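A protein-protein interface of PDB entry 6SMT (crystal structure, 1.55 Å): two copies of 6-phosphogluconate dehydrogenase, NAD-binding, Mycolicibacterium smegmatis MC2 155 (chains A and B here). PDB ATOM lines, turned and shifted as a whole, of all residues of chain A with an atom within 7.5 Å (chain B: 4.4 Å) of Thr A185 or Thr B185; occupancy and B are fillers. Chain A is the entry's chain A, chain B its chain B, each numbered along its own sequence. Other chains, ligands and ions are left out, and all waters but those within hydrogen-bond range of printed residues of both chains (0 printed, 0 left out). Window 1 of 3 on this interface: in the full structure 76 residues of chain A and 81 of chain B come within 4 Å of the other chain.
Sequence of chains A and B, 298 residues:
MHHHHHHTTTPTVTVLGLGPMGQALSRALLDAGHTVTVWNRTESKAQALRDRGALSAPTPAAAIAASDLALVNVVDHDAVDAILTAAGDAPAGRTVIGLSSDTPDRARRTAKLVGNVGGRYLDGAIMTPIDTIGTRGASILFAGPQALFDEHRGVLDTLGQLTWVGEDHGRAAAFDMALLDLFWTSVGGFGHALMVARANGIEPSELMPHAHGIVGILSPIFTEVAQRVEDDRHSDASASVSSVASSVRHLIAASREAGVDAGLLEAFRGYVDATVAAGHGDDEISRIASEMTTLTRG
Asp A181 touches Leu B265, and with the chains exchanged Leu A265 touches Asp B181.
Thr A185 touches Gly B189, and with the chains exchanged Gly A189 touches Thr B185.
Thr A185 touches Leu B264, and with the chains exchanged Leu A264 touches Thr B185.
Leu A264 touches its own counterpart, Leu B264.
Of the 21 pairs that touch across the chains among the printed residues, 13 have their exchanged pair printed and touching as well.
OG of Ser A186 sits at hydrogen-bond distance from OG of Ser B186.
ND1 of His A192 lies within hydrogen-bond range of OD2 of Asp B181 (2.5 Å).
The backbone NH of Ala A193 sits close to the side-chain carboxylate of Asp B181, at 3.4 Å.
OG1 of Thr A185 sits at hydrogen-bond distance from O of Asp A181 (2.8 Å).
The backbone carbonyl oxygen (O) of Leu A182 sits at hydrogen-bond distance from the side-chain hydroxyl (OG) of Ser A186 (2.8 Å).
OG1 of Thr B185 lies within hydrogen-bond range of O of Asp B181, 2.7 Å away.
The backbone carbonyl oxygen of Leu B182 sits at hydrogen-bond distance from the side-chain hydroxyl of Ser B186, 2.8 Å away.
Of the printed residues of chain B, Thr A185 touches Thr B185, Gly B189, Leu B264 and Leu B265.
Thr B185 touches just these residues of chain A: Thr A185, Gly A189, Leu A264 and Leu A265.
Printed residues of chain A within 4 Å of Leu B264: Thr A185, Leu A264 and Phe A268.
Of the printed residues of chain B, Gly A189 touches Asp B181 and Thr B185.
Of the printed residues of chain B, Leu A265 touches Asp B181 and Thr B185.
Printed residues of chain B within 4 Å of Asp A181: Leu B265 (3.7 Å).
Of the printed residues of chain B, His A192 touches Asp B181.
The nearest residue of chain A that does not touch Thr B185 is Gly A188 (4.7 Å).
The nearest printed residue of chain B that does not touch Asp A181 is Gly B189 (4.01 Å).
Of the 20 printed residues of chain A, 12 touch a printed residue of chain B.
Printed residues of chain A that touch a printed residue of chain B: Asp A181, Leu A182, Thr A185, Ser A186, Gly A189, Phe A190, His A192, Ala A193, Leu A251, Leu A264, Leu A265 and Phe A268.
Along chain A the printed residues that touch a printed residue of chain B span positions 181 to 268.
Of the 11 printed residues of chain B, 9 touch a printed residue of chain A.
Hydrophobic or aromatic side chains of chain B within 4 Å of the printed part of chain A: Leu B182, Trp B184, Leu B264 and Leu B265.
Among the printed residues, 21 pairs touch across the chains.
Among the printed residues, no Asp or Glu carboxylate lies within 4 Å of a Lys or Arg side-chain nitrogen of the other chain.
OD1 of Asp A181 touches CD1 of Leu B265, at 3.7 Å.
CG2 of Thr A185 touches CA of Gly B189, at 3.6 Å.
Thr A185 touches Leu B264.
Ser A186 touches Leu B182 (O to CD1, 3.96 Å).
Thr B185 touches Gly A189.
Leu B182 touches Phe A190.
Asp B181 touches Leu A251 (N to CD1, 3.9 Å).
Leu A265 touches Thr B185 (CD2 to OG1, 3.8 Å).
CZ of Phe A268 touches CE3 of Trp B184, at 3.9 Å.
CE1 of Phe A268 touches CA of Gly B188 (3.7 Å).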
ATOM      1  N   LEU A 179     -14.288 -21.756  22.332  1.00  0.00           N
ATOM      2  CA  LEU A 179     -14.044 -20.469  22.948  1.00  0.00           C
ATOM      3  C   LEU A 179     -14.125 -19.343  21.921  1.00  0.00           C
ATOM      4  O   LEU A 179     -14.681 -18.273  22.212  1.00  0.00           O
ATOM      5  CB  LEU A 179     -12.710 -20.508  23.682  1.00  0.00           C
ATOM      6  CG  LEU A 179     -12.643 -21.503  24.812  1.00  0.00           C
ATOM      7  CD1 LEU A 179     -11.232 -21.650  25.261  1.00  0.00           C
ATOM      8  CD2 LEU A 179     -13.534 -21.084  25.984  1.00  0.00           C
ATOM      9  N   LEU A 180     -13.605 -19.554  20.704  1.00  0.00           N
ATOM     10  CA  LEU A 180     -13.669 -18.510  19.648  1.00  0.00           C
ATOM     11  C   LEU A 180     -15.112 -18.427  19.136  1.00  0.00           C
ATOM     12  O   LEU A 180     -15.474 -17.309  18.707  1.00  0.00           O
ATOM     13  CB  LEU A 180     -12.739 -18.900  18.497  1.00  0.00           C
ATOM     14  CG  LEU A 180     -11.255 -18.779  18.842  1.00  0.00           C
ATOM     15  CD1 LEU A 180     -10.442 -19.309  17.640  1.00  0.00           C
ATOM     16  CD2 LEU A 180     -10.826 -17.404  19.205  1.00  0.00           C
ATOM     17  N   ASP A 181     -15.887 -19.487  19.138  1.00  0.00           N
ATOM     18  CA  ASP A 181     -17.308 -19.444  18.796  1.00  0.00           C
ATOM     19  C   ASP A 181     -17.989 -18.486  19.762  1.00  0.00           C
ATOM     20  O   ASP A 181     -18.670 -17.501  19.341  1.00  0.00           O
ATOM     21  CB  ASP A 181     -17.840 -20.839  18.877  1.00  0.00           C
ATOM     22  CG  ASP A 181     -19.294 -21.085  18.785  1.00  0.00           C
ATOM     23  OD1 ASP A 181     -19.988 -20.070  18.347  1.00  0.00           O
ATOM     24  OD2 ASP A 181     -19.709 -22.247  19.039  1.00  0.00           O
ATOM     25  N   LEU A 182     -17.788 -18.663  21.036  1.00  0.00           N
ATOM     26  CA  LEU A 182     -18.376 -17.719  22.033  1.00  0.00           C
ATOM     27  C   LEU A 182     -17.889 -16.326  21.761  1.00  0.00           C
ATOM     28  O   LEU A 182     -18.671 -15.346  21.741  1.00  0.00           O
ATOM     29  CB  LEU A 182     -17.957 -18.181  23.403  1.00  0.00           C
ATOM     30  CG  LEU A 182     -18.229 -17.233  24.538  1.00  0.00           C
ATOM     31  CD1 LEU A 182     -19.746 -16.912  24.629  1.00  0.00           C
ATOM     32  CD2 LEU A 182     -17.659 -17.765  25.840  1.00  0.00           C
ATOM     33  N   PHE A 183     -16.588 -16.119  21.578  1.00  0.00           N
ATOM     34  CA  PHE A 183     -16.020 -14.807  21.414  1.00  0.00           C
ATOM     35  C   PHE A 183     -16.579 -14.104  20.163  1.00  0.00           C
ATOM     36  O   PHE A 183     -17.056 -12.970  20.291  1.00  0.00           O
ATOM     37  CB  PHE A 183     -14.495 -14.905  21.347  1.00  0.00           C
ATOM     38  CG  PHE A 183     -13.845 -13.603  21.082  1.00  0.00           C
ATOM     39  CD1 PHE A 183     -13.705 -12.656  22.092  1.00  0.00           C
ATOM     40  CD2 PHE A 183     -13.425 -13.260  19.768  1.00  0.00           C
ATOM     41  CE1 PHE A 183     -13.215 -11.385  21.840  1.00  0.00           C
ATOM     42  CE2 PHE A 183     -12.860 -12.038  19.563  1.00  0.00           C
ATOM     43  CZ  PHE A 183     -12.785 -11.061  20.557  1.00  0.00           C
ATOM     44  N   TRP A 184     -16.462 -14.694  19.005  1.00  0.00           N
ATOM     45  CA  TRP A 184     -16.821 -14.001  17.753  1.00  0.00           C
ATOM     46  C   TRP A 184     -18.332 -13.838  17.709  1.00  0.00           C
ATOM     47  O   TRP A 184     -18.749 -12.791  17.135  1.00  0.00           O
ATOM     48  CB  TRP A 184     -16.275 -14.736  16.504  1.00  0.00           C
ATOM     49  CG  TRP A 184     -14.799 -14.521  16.410  1.00  0.00           C
ATOM     50  CD1 TRP A 184     -13.838 -15.522  16.487  1.00  0.00           C
ATOM     51  CD2 TRP A 184     -14.057 -13.325  16.204  1.00  0.00           C
ATOM     52  NE1 TRP A 184     -12.594 -14.985  16.375  1.00  0.00           N
ATOM     53  CE2 TRP A 184     -12.657 -13.636  16.194  1.00  0.00           C
ATOM     54  CE3 TRP A 184     -14.427 -11.979  16.055  1.00  0.00           C
ATOM     55  CZ2 TRP A 184     -11.706 -12.670  16.060  1.00  0.00           C
ATOM     56  CZ3 TRP A 184     -13.465 -11.035  15.868  1.00  0.00           C
ATOM     57  CH2 TRP A 184     -12.099 -11.374  15.891  1.00  0.00           C
ATOM     58  N   THR A 185     -19.121 -14.731  18.201  1.00  0.00           N
ATOM     59  CA  THR A 185     -20.589 -14.557  18.188  1.00  0.00           C
ATOM     60  C   THR A 185     -20.937 -13.336  19.042  1.00  0.00           C
ATOM     61  O   THR A 185     -21.763 -12.492  18.645  1.00  0.00           O
ATOM     62  CB  THR A 185     -21.293 -15.809  18.661  1.00  0.00           C
ATOM     63  OG1 THR A 185     -20.943 -16.930  17.826  1.00  0.00           O
ATOM     64  CG2 THR A 185     -22.785 -15.659  18.616  1.00  0.00           C
ATOM     65  N   SER A 186     -20.248 -13.152  20.164  1.00  0.00           N
ATOM     66  CA  SER A 186     -20.458 -11.987  21.060  1.00  0.00           C
ATOM     67  C   SER A 186     -20.046 -10.688  20.355  1.00  0.00           C
ATOM     68  O   SER A 186     -20.696  -9.579  20.377  1.00  0.00           O
ATOM     69  CB  SER A 186     -19.719 -12.202  22.353  1.00  0.00           C
ATOM     70  OG  SER A 186     -20.177 -13.378  23.008  1.00  0.00           O
ATOM     71  N   VAL A 187     -18.888 -10.746  19.687  1.00  0.00           N
ATOM     72  CA  VAL A 187     -18.408  -9.607  18.879  1.00  0.00           C
ATOM     73  C   VAL A 187     -19.468  -9.245  17.802  1.00  0.00           C
ATOM     74  O   VAL A 187     -19.723  -8.049  17.546  1.00  0.00           O
ATOM     75  CB  VAL A 187     -17.037  -9.854  18.260  1.00  0.00           C
ATOM     76  CG1 VAL A 187     -16.682  -8.818  17.227  1.00  0.00           C
ATOM     77  CG2 VAL A 187     -15.997  -9.874  19.367  1.00  0.00           C
ATOM     78  N   GLY A 188     -20.021 -10.222  17.099  1.00  0.00           N
ATOM     79  CA  GLY A 188     -21.078  -9.969  16.118  1.00  0.00           C
ATOM     80  C   GLY A 188     -22.277  -9.323  16.796  1.00  0.00           C
ATOM     81  O   GLY A 188     -22.816  -8.356  16.199  1.00  0.00           O
ATOM     82  N   GLY A 189     -22.662  -9.784  17.954  1.00  0.00           N
ATOM     83  CA  GLY A 189     -23.781  -9.134  18.629  1.00  0.00           C
ATOM     84  C   GLY A 189     -23.465  -7.720  19.047  1.00  0.00           C
ATOM     85  O   GLY A 189     -24.315  -6.806  18.874  1.00  0.00           O
ATOM     86  N   PHE A 190     -22.256  -7.474  19.517  1.00  0.00           N
ATOM     87  CA  PHE A 190     -21.866  -6.117  19.913  1.00  0.00           C
ATOM     88  C   PHE A 190     -21.857  -5.156  18.751  1.00  0.00           C
ATOM     89  O   PHE A 190     -22.366  -4.072  18.810  1.00  0.00           O
ATOM     90  CB  PHE A 190     -20.486  -6.165  20.579  1.00  0.00           C
ATOM     91  CG  PHE A 190     -20.029  -4.808  21.050  1.00  0.00           C
ATOM     92  CD1 PHE A 190     -20.616  -4.183  22.104  1.00  0.00           C
ATOM     93  CD2 PHE A 190     -18.997  -4.157  20.383  1.00  0.00           C
ATOM     94  CE1 PHE A 190     -20.224  -2.908  22.525  1.00  0.00           C
ATOM     95  CE2 PHE A 190     -18.568  -2.928  20.805  1.00  0.00           C
ATOM     96  CZ  PHE A 190     -19.182  -2.313  21.871  1.00  0.00           C
ATOM     97  N   GLY A 191     -21.272  -5.514  17.610  1.00  0.00           N
ATOM     98  CA  GLY A 191     -21.222  -4.612  16.477  1.00  0.00           C
ATOM     99  C   GLY A 191     -22.640  -4.330  15.973  1.00  0.00           C
ATOM    100  O   GLY A 191     -22.890  -3.218  15.591  1.00  0.00           O
ATOM    101  N   HIS A 192     -23.485  -5.346  15.956  1.00  0.00           N
ATOM    102  CA  HIS A 192     -24.904  -5.157  15.564  1.00  0.00           C
ATOM    103  C   HIS A 192     -25.583  -4.191  16.536  1.00  0.00           C
ATOM    104  O   HIS A 192     -26.304  -3.276  16.084  1.00  0.00           O
ATOM    105  CB  HIS A 192     -25.566  -6.521  15.514  1.00  0.00           C
ATOM    106  CG  HIS A 192     -26.946  -6.515  15.011  1.00  0.00           C
ATOM    107  ND1 HIS A 192     -27.999  -6.270  15.867  1.00  0.00           N
ATOM    108  CD2 HIS A 192     -27.432  -6.667  13.751  1.00  0.00           C
ATOM    109  CE1 HIS A 192     -29.103  -6.253  15.092  1.00  0.00           C
ATOM    110  NE2 HIS A 192     -28.799  -6.446  13.796  1.00  0.00           N
ATOM    111  N   ALA A 193     -25.357  -4.383  17.812  1.00  0.00           N
ATOM    112  CA  ALA A 193     -26.013  -3.556  18.838  1.00  0.00           C
ATOM    113  C   ALA A 193     -25.600  -2.101  18.624  1.00  0.00           C
ATOM    114  O   ALA A 193     -26.412  -1.232  18.745  1.00  0.00           O
ATOM    115  CB  ALA A 193     -25.657  -4.037  20.201  1.00  0.00           C
ATOM    116  N   PHE A 222     -23.792 -17.741  32.485  1.00  0.00           N
ATOM    117  CA  PHE A 222     -23.150 -18.876  31.809  1.00  0.00           C
ATOM    118  C   PHE A 222     -22.886 -20.022  32.807  1.00  0.00           C
ATOM    119  O   PHE A 222     -23.051 -21.162  32.422  1.00  0.00           O
ATOM    120  CB  PHE A 222     -21.867 -18.389  31.126  1.00  0.00           C
ATOM    121  CG  PHE A 222     -22.013 -17.498  29.916  1.00  0.00           C
ATOM    122  CD1 PHE A 222     -23.223 -17.177  29.335  1.00  0.00           C
ATOM    123  CD2 PHE A 222     -20.883 -16.957  29.343  1.00  0.00           C
ATOM    124  CE1 PHE A 222     -23.315 -16.346  28.225  1.00  0.00           C
ATOM    125  CE2 PHE A 222     -20.981 -16.126  28.223  1.00  0.00           C
ATOM    126  CZ  PHE A 222     -22.177 -15.849  27.662  1.00  0.00           C
ATOM    127  N   LEU A 251     -36.486  -7.403  19.042  1.00  0.00           N
ATOM    128  CA  LEU A 251     -35.115  -7.070  18.664  1.00  0.00           C
ATOM    129  C   LEU A 251     -34.973  -7.123  17.130  1.00  0.00           C
ATOM    130  O   LEU A 251     -34.359  -6.227  16.562  1.00  0.00           O
ATOM    131  CB  LEU A 251     -34.102  -8.033  19.323  1.00  0.00           C
ATOM    132  CG  LEU A 251     -34.211  -8.183  20.846  1.00  0.00           C
ATOM    133  CD1 LEU A 251     -33.133  -9.104  21.389  1.00  0.00           C
ATOM    134  CD2 LEU A 251     -34.099  -6.862  21.512  1.00  0.00           C
ATOM    135  N   LEU A 264     -28.012 -12.828  12.862  1.00  0.00           N
ATOM    136  CA  LEU A 264     -27.701 -13.591  14.074  1.00  0.00           C
ATOM    137  C   LEU A 264     -28.947 -13.780  14.936  1.00  0.00           C
ATOM    138  O   LEU A 264     -29.222 -14.936  15.367  1.00  0.00           O
ATOM    139  CB  LEU A 264     -26.534 -12.953  14.855  1.00  0.00           C
ATOM    140  CG  LEU A 264     -25.130 -13.395  14.340  1.00  0.00           C
ATOM    141  CD1 LEU A 264     -24.704 -12.580  13.187  1.00  0.00           C
ATOM    142  CD2 LEU A 264     -24.071 -13.290  15.421  1.00  0.00           C
ATOM    143  N   LEU A 265     -29.711 -12.686  15.164  1.00  0.00           N
ATOM    144  CA  LEU A 265     -30.934 -12.861  15.951  1.00  0.00           C
ATOM    145  C   LEU A 265     -31.966 -13.772  15.257  1.00  0.00           C
ATOM    146  O   LEU A 265     -32.669 -14.447  15.964  1.00  0.00           O
ATOM    147  CB  LEU A 265     -31.502 -11.482  16.222  1.00  0.00           C
ATOM    148  CG  LEU A 265     -30.727 -10.596  17.199  1.00  0.00           C
ATOM    149  CD1 LEU A 265     -31.140  -9.150  17.077  1.00  0.00           C
ATOM    150  CD2 LEU A 265     -30.938 -11.090  18.558  1.00  0.00           C
ATOM    151  N   PHE A 268     -31.015 -17.231  16.002  1.00  0.00           N
ATOM    152  CA  PHE A 268     -31.370 -17.502  17.404  1.00  0.00           C
ATOM    153  C   PHE A 268     -32.870 -17.757  17.569  1.00  0.00           C
ATOM    154  O   PHE A 268     -33.317 -18.676  18.252  1.00  0.00           O
ATOM    155  CB  PHE A 268     -30.848 -16.366  18.318  1.00  0.00           C
ATOM    156  CG  PHE A 268     -31.009 -16.621  19.783  1.00  0.00           C
ATOM    157  CD1 PHE A 268     -30.334 -17.683  20.396  1.00  0.00           C
ATOM    158  CD2 PHE A 268     -31.848 -15.882  20.598  1.00  0.00           C
ATOM    159  CE1 PHE A 268     -30.472 -17.985  21.724  1.00  0.00           C
ATOM    160  CE2 PHE A 268     -31.972 -16.171  21.942  1.00  0.00           C
ATOM    161  CZ  PHE A 268     -31.268 -17.167  22.510  1.00  0.00           C
ATOM    162  N   ASP B 181     -29.913  -7.295  22.486  1.00  0.00           N
ATOM    163  CA  ASP B 181     -29.279  -7.807  21.261  1.00  0.00           C
ATOM    164  C   ASP B 181     -27.899  -8.374  21.624  1.00  0.00           C
ATOM    165  O   ASP B 181     -27.604  -9.545  21.327  1.00  0.00           O
ATOM    166  CB  ASP B 181     -29.227  -6.688  20.255  1.00  0.00           C
ATOM    167  CG  ASP B 181     -28.498  -6.902  19.006  1.00  0.00           C
ATOM    168  OD1 ASP B 181     -28.104  -8.071  18.738  1.00  0.00           O
ATOM    169  OD2 ASP B 181     -28.344  -5.915  18.277  1.00  0.00           O
ATOM    170  N   LEU B 182     -27.087  -7.558  22.266  1.00  0.00           N
ATOM    171  CA  LEU B 182     -25.750  -8.046  22.731  1.00  0.00           C
ATOM    172  C   LEU B 182     -25.924  -9.279  23.595  1.00  0.00           C
ATOM    173  O   LEU B 182     -25.210 -10.287  23.414  1.00  0.00           O
ATOM    174  CB  LEU B 182     -25.064  -6.907  23.445  1.00  0.00           C
ATOM    175  CG  LEU B 182     -23.815  -7.287  24.214  1.00  0.00           C
ATOM    176  CD1 LEU B 182     -22.776  -7.847  23.272  1.00  0.00           C
ATOM    177  CD2 LEU B 182     -23.307  -6.162  25.047  1.00  0.00           C
ATOM    178  N   PHE B 183     -26.781  -9.185  24.593  1.00  0.00           N
ATOM    179  CA  PHE B 183     -26.934 -10.246  25.577  1.00  0.00           C
ATOM    180  C   PHE B 183     -27.350 -11.568  24.927  1.00  0.00           C
ATOM    181  O   PHE B 183     -26.707 -12.621  25.102  1.00  0.00           O
ATOM    182  CB  PHE B 183     -27.940  -9.851  26.626  1.00  0.00           C
ATOM    183  CG  PHE B 183     -28.211 -10.963  27.609  1.00  0.00           C
ATOM    184  CD1 PHE B 183     -27.278 -11.340  28.549  1.00  0.00           C
ATOM    185  CD2 PHE B 183     -29.380 -11.708  27.533  1.00  0.00           C
ATOM    186  CE1 PHE B 183     -27.516 -12.419  29.394  1.00  0.00           C
ATOM    187  CE2 PHE B 183     -29.642 -12.760  28.388  1.00  0.00           C
ATOM    188  CZ  PHE B 183     -28.704 -13.115  29.324  1.00  0.00           C
ATOM    189  N   TRP B 184     -28.492 -11.561  24.196  1.00  0.00           N
ATOM    190  CA  TRP B 184     -29.016 -12.841  23.670  1.00  0.00           C
ATOM    191  C   TRP B 184     -28.102 -13.389  22.595  1.00  0.00           C
ATOM    192  O   TRP B 184     -28.058 -14.635  22.440  1.00  0.00           O
ATOM    193  CB  TRP B 184     -30.458 -12.660  23.187  1.00  0.00           C
ATOM    194  CG  TRP B 184     -31.436 -12.513  24.313  1.00  0.00           C
ATOM    195  CD1 TRP B 184     -32.193 -11.398  24.614  1.00  0.00           C
ATOM    196  CD2 TRP B 184     -31.704 -13.466  25.363  1.00  0.00           C
ATOM    197  NE1 TRP B 184     -32.899 -11.624  25.762  1.00  0.00           N
ATOM    198  CE2 TRP B 184     -32.677 -12.892  26.214  1.00  0.00           C
ATOM    199  CE3 TRP B 184     -31.271 -14.789  25.599  1.00  0.00           C
ATOM    200  CZ2 TRP B 184     -33.157 -13.550  27.337  1.00  0.00           C
ATOM    201  CZ3 TRP B 184     -31.754 -15.412  26.735  1.00  0.00           C
ATOM    202  CH2 TRP B 184     -32.708 -14.825  27.568  1.00  0.00           C
ATOM    203  N   THR B 185     -27.474 -12.530  21.777  1.00  0.00           N
ATOM    204  CA  THR B 185     -26.540 -13.028  20.772  1.00  0.00           C
ATOM    205  C   THR B 185     -25.434 -13.791  21.484  1.00  0.00           C
ATOM    206  O   THR B 185     -25.027 -14.871  21.065  1.00  0.00           O
ATOM    207  CB  THR B 185     -26.052 -11.920  19.881  1.00  0.00           C
ATOM    208  OG1 THR B 185     -27.181 -11.261  19.247  1.00  0.00           O
ATOM    209  CG2 THR B 185     -25.149 -12.451  18.802  1.00  0.00           C
ATOM    210  N   SER B 186     -24.932 -13.195  22.576  1.00  0.00           N
ATOM    211  CA  SER B 186     -23.855 -13.821  23.375  1.00  0.00           C
ATOM    212  C   SER B 186     -24.333 -15.153  23.945  1.00  0.00           C
ATOM    213  O   SER B 186     -23.584 -16.161  23.898  1.00  0.00           O
ATOM    214  CB  SER B 186     -23.398 -12.846  24.451  1.00  0.00           C
ATOM    215  OG  SER B 186     -22.855 -11.646  23.883  1.00  0.00           O
ATOM    216  N   VAL B 187     -25.533 -15.210  24.510  1.00  0.00           N
ATOM    217  CA  VAL B 187     -26.126 -16.447  25.047  1.00  0.00           C
ATOM    218  C   VAL B 187     -26.241 -17.468  23.924  1.00  0.00           C
ATOM    219  O   VAL B 187     -25.959 -18.659  24.152  1.00  0.00           O
ATOM    220  CB  VAL B 187     -27.497 -16.187  25.684  1.00  0.00           C
ATOM    221  CG1 VAL B 187     -28.291 -17.469  25.943  1.00  0.00           C
ATOM    222  CG2 VAL B 187     -27.251 -15.404  26.936  1.00  0.00           C
ATOM    223  N   GLY B 188     -26.675 -17.095  22.743  1.00  0.00           N
ATOM    224  CA  GLY B 188     -26.732 -18.016  21.572  1.00  0.00           C
ATOM    225  C   GLY B 188     -25.365 -18.582  21.284  1.00  0.00           C
ATOM    226  O   GLY B 188     -25.224 -19.822  21.076  1.00  0.00           O
ATOM    227  N   GLY B 189     -24.333 -17.745  21.290  1.00  0.00           N
ATOM    228  CA  GLY B 189     -22.945 -18.197  21.101  1.00  0.00           C
ATOM    229  C   GLY B 189     -22.536 -19.168  22.169  1.00  0.00           C
ATOM    230  O   GLY B 189     -21.873 -20.192  21.883  1.00  0.00           O
ATOM    231  N   LEU B 264     -25.592 -18.779  13.507  1.00  0.00           N
ATOM    232  CA  LEU B 264     -25.100 -17.482  13.951  1.00  0.00           C
ATOM    233  C   LEU B 264     -23.748 -17.198  13.305  1.00  0.00           C
ATOM    234  O   LEU B 264     -23.511 -16.104  12.770  1.00  0.00           O
ATOM    235  CB  LEU B 264     -25.042 -17.341  15.475  1.00  0.00           C
ATOM    236  CG  LEU B 264     -26.369 -16.853  16.123  1.00  0.00           C
ATOM    237  CD1 LEU B 264     -27.261 -18.011  16.204  1.00  0.00           C
ATOM    238  CD2 LEU B 264     -26.157 -16.167  17.429  1.00  0.00           C
ATOM    239  N   LEU B 265     -22.836 -18.166  13.304  1.00  0.00           N
ATOM    240  CA  LEU B 265     -21.522 -17.944  12.692  1.00  0.00           C
ATOM    241  C   LEU B 265     -21.625 -17.763  11.178  1.00  0.00           C
ATOM    242  O   LEU B 265     -20.825 -17.013  10.608  1.00  0.00           O
ATOM    243  CB  LEU B 265     -20.567 -19.112  12.982  1.00  0.00           C
ATOM    244  CG  LEU B 265     -20.139 -19.253  14.439  1.00  0.00           C
ATOM    245  CD1 LEU B 265     -19.701 -20.687  14.697  1.00  0.00           C
ATOM    246  CD2 LEU B 265     -19.085 -18.252  14.748  1.00  0.00           C
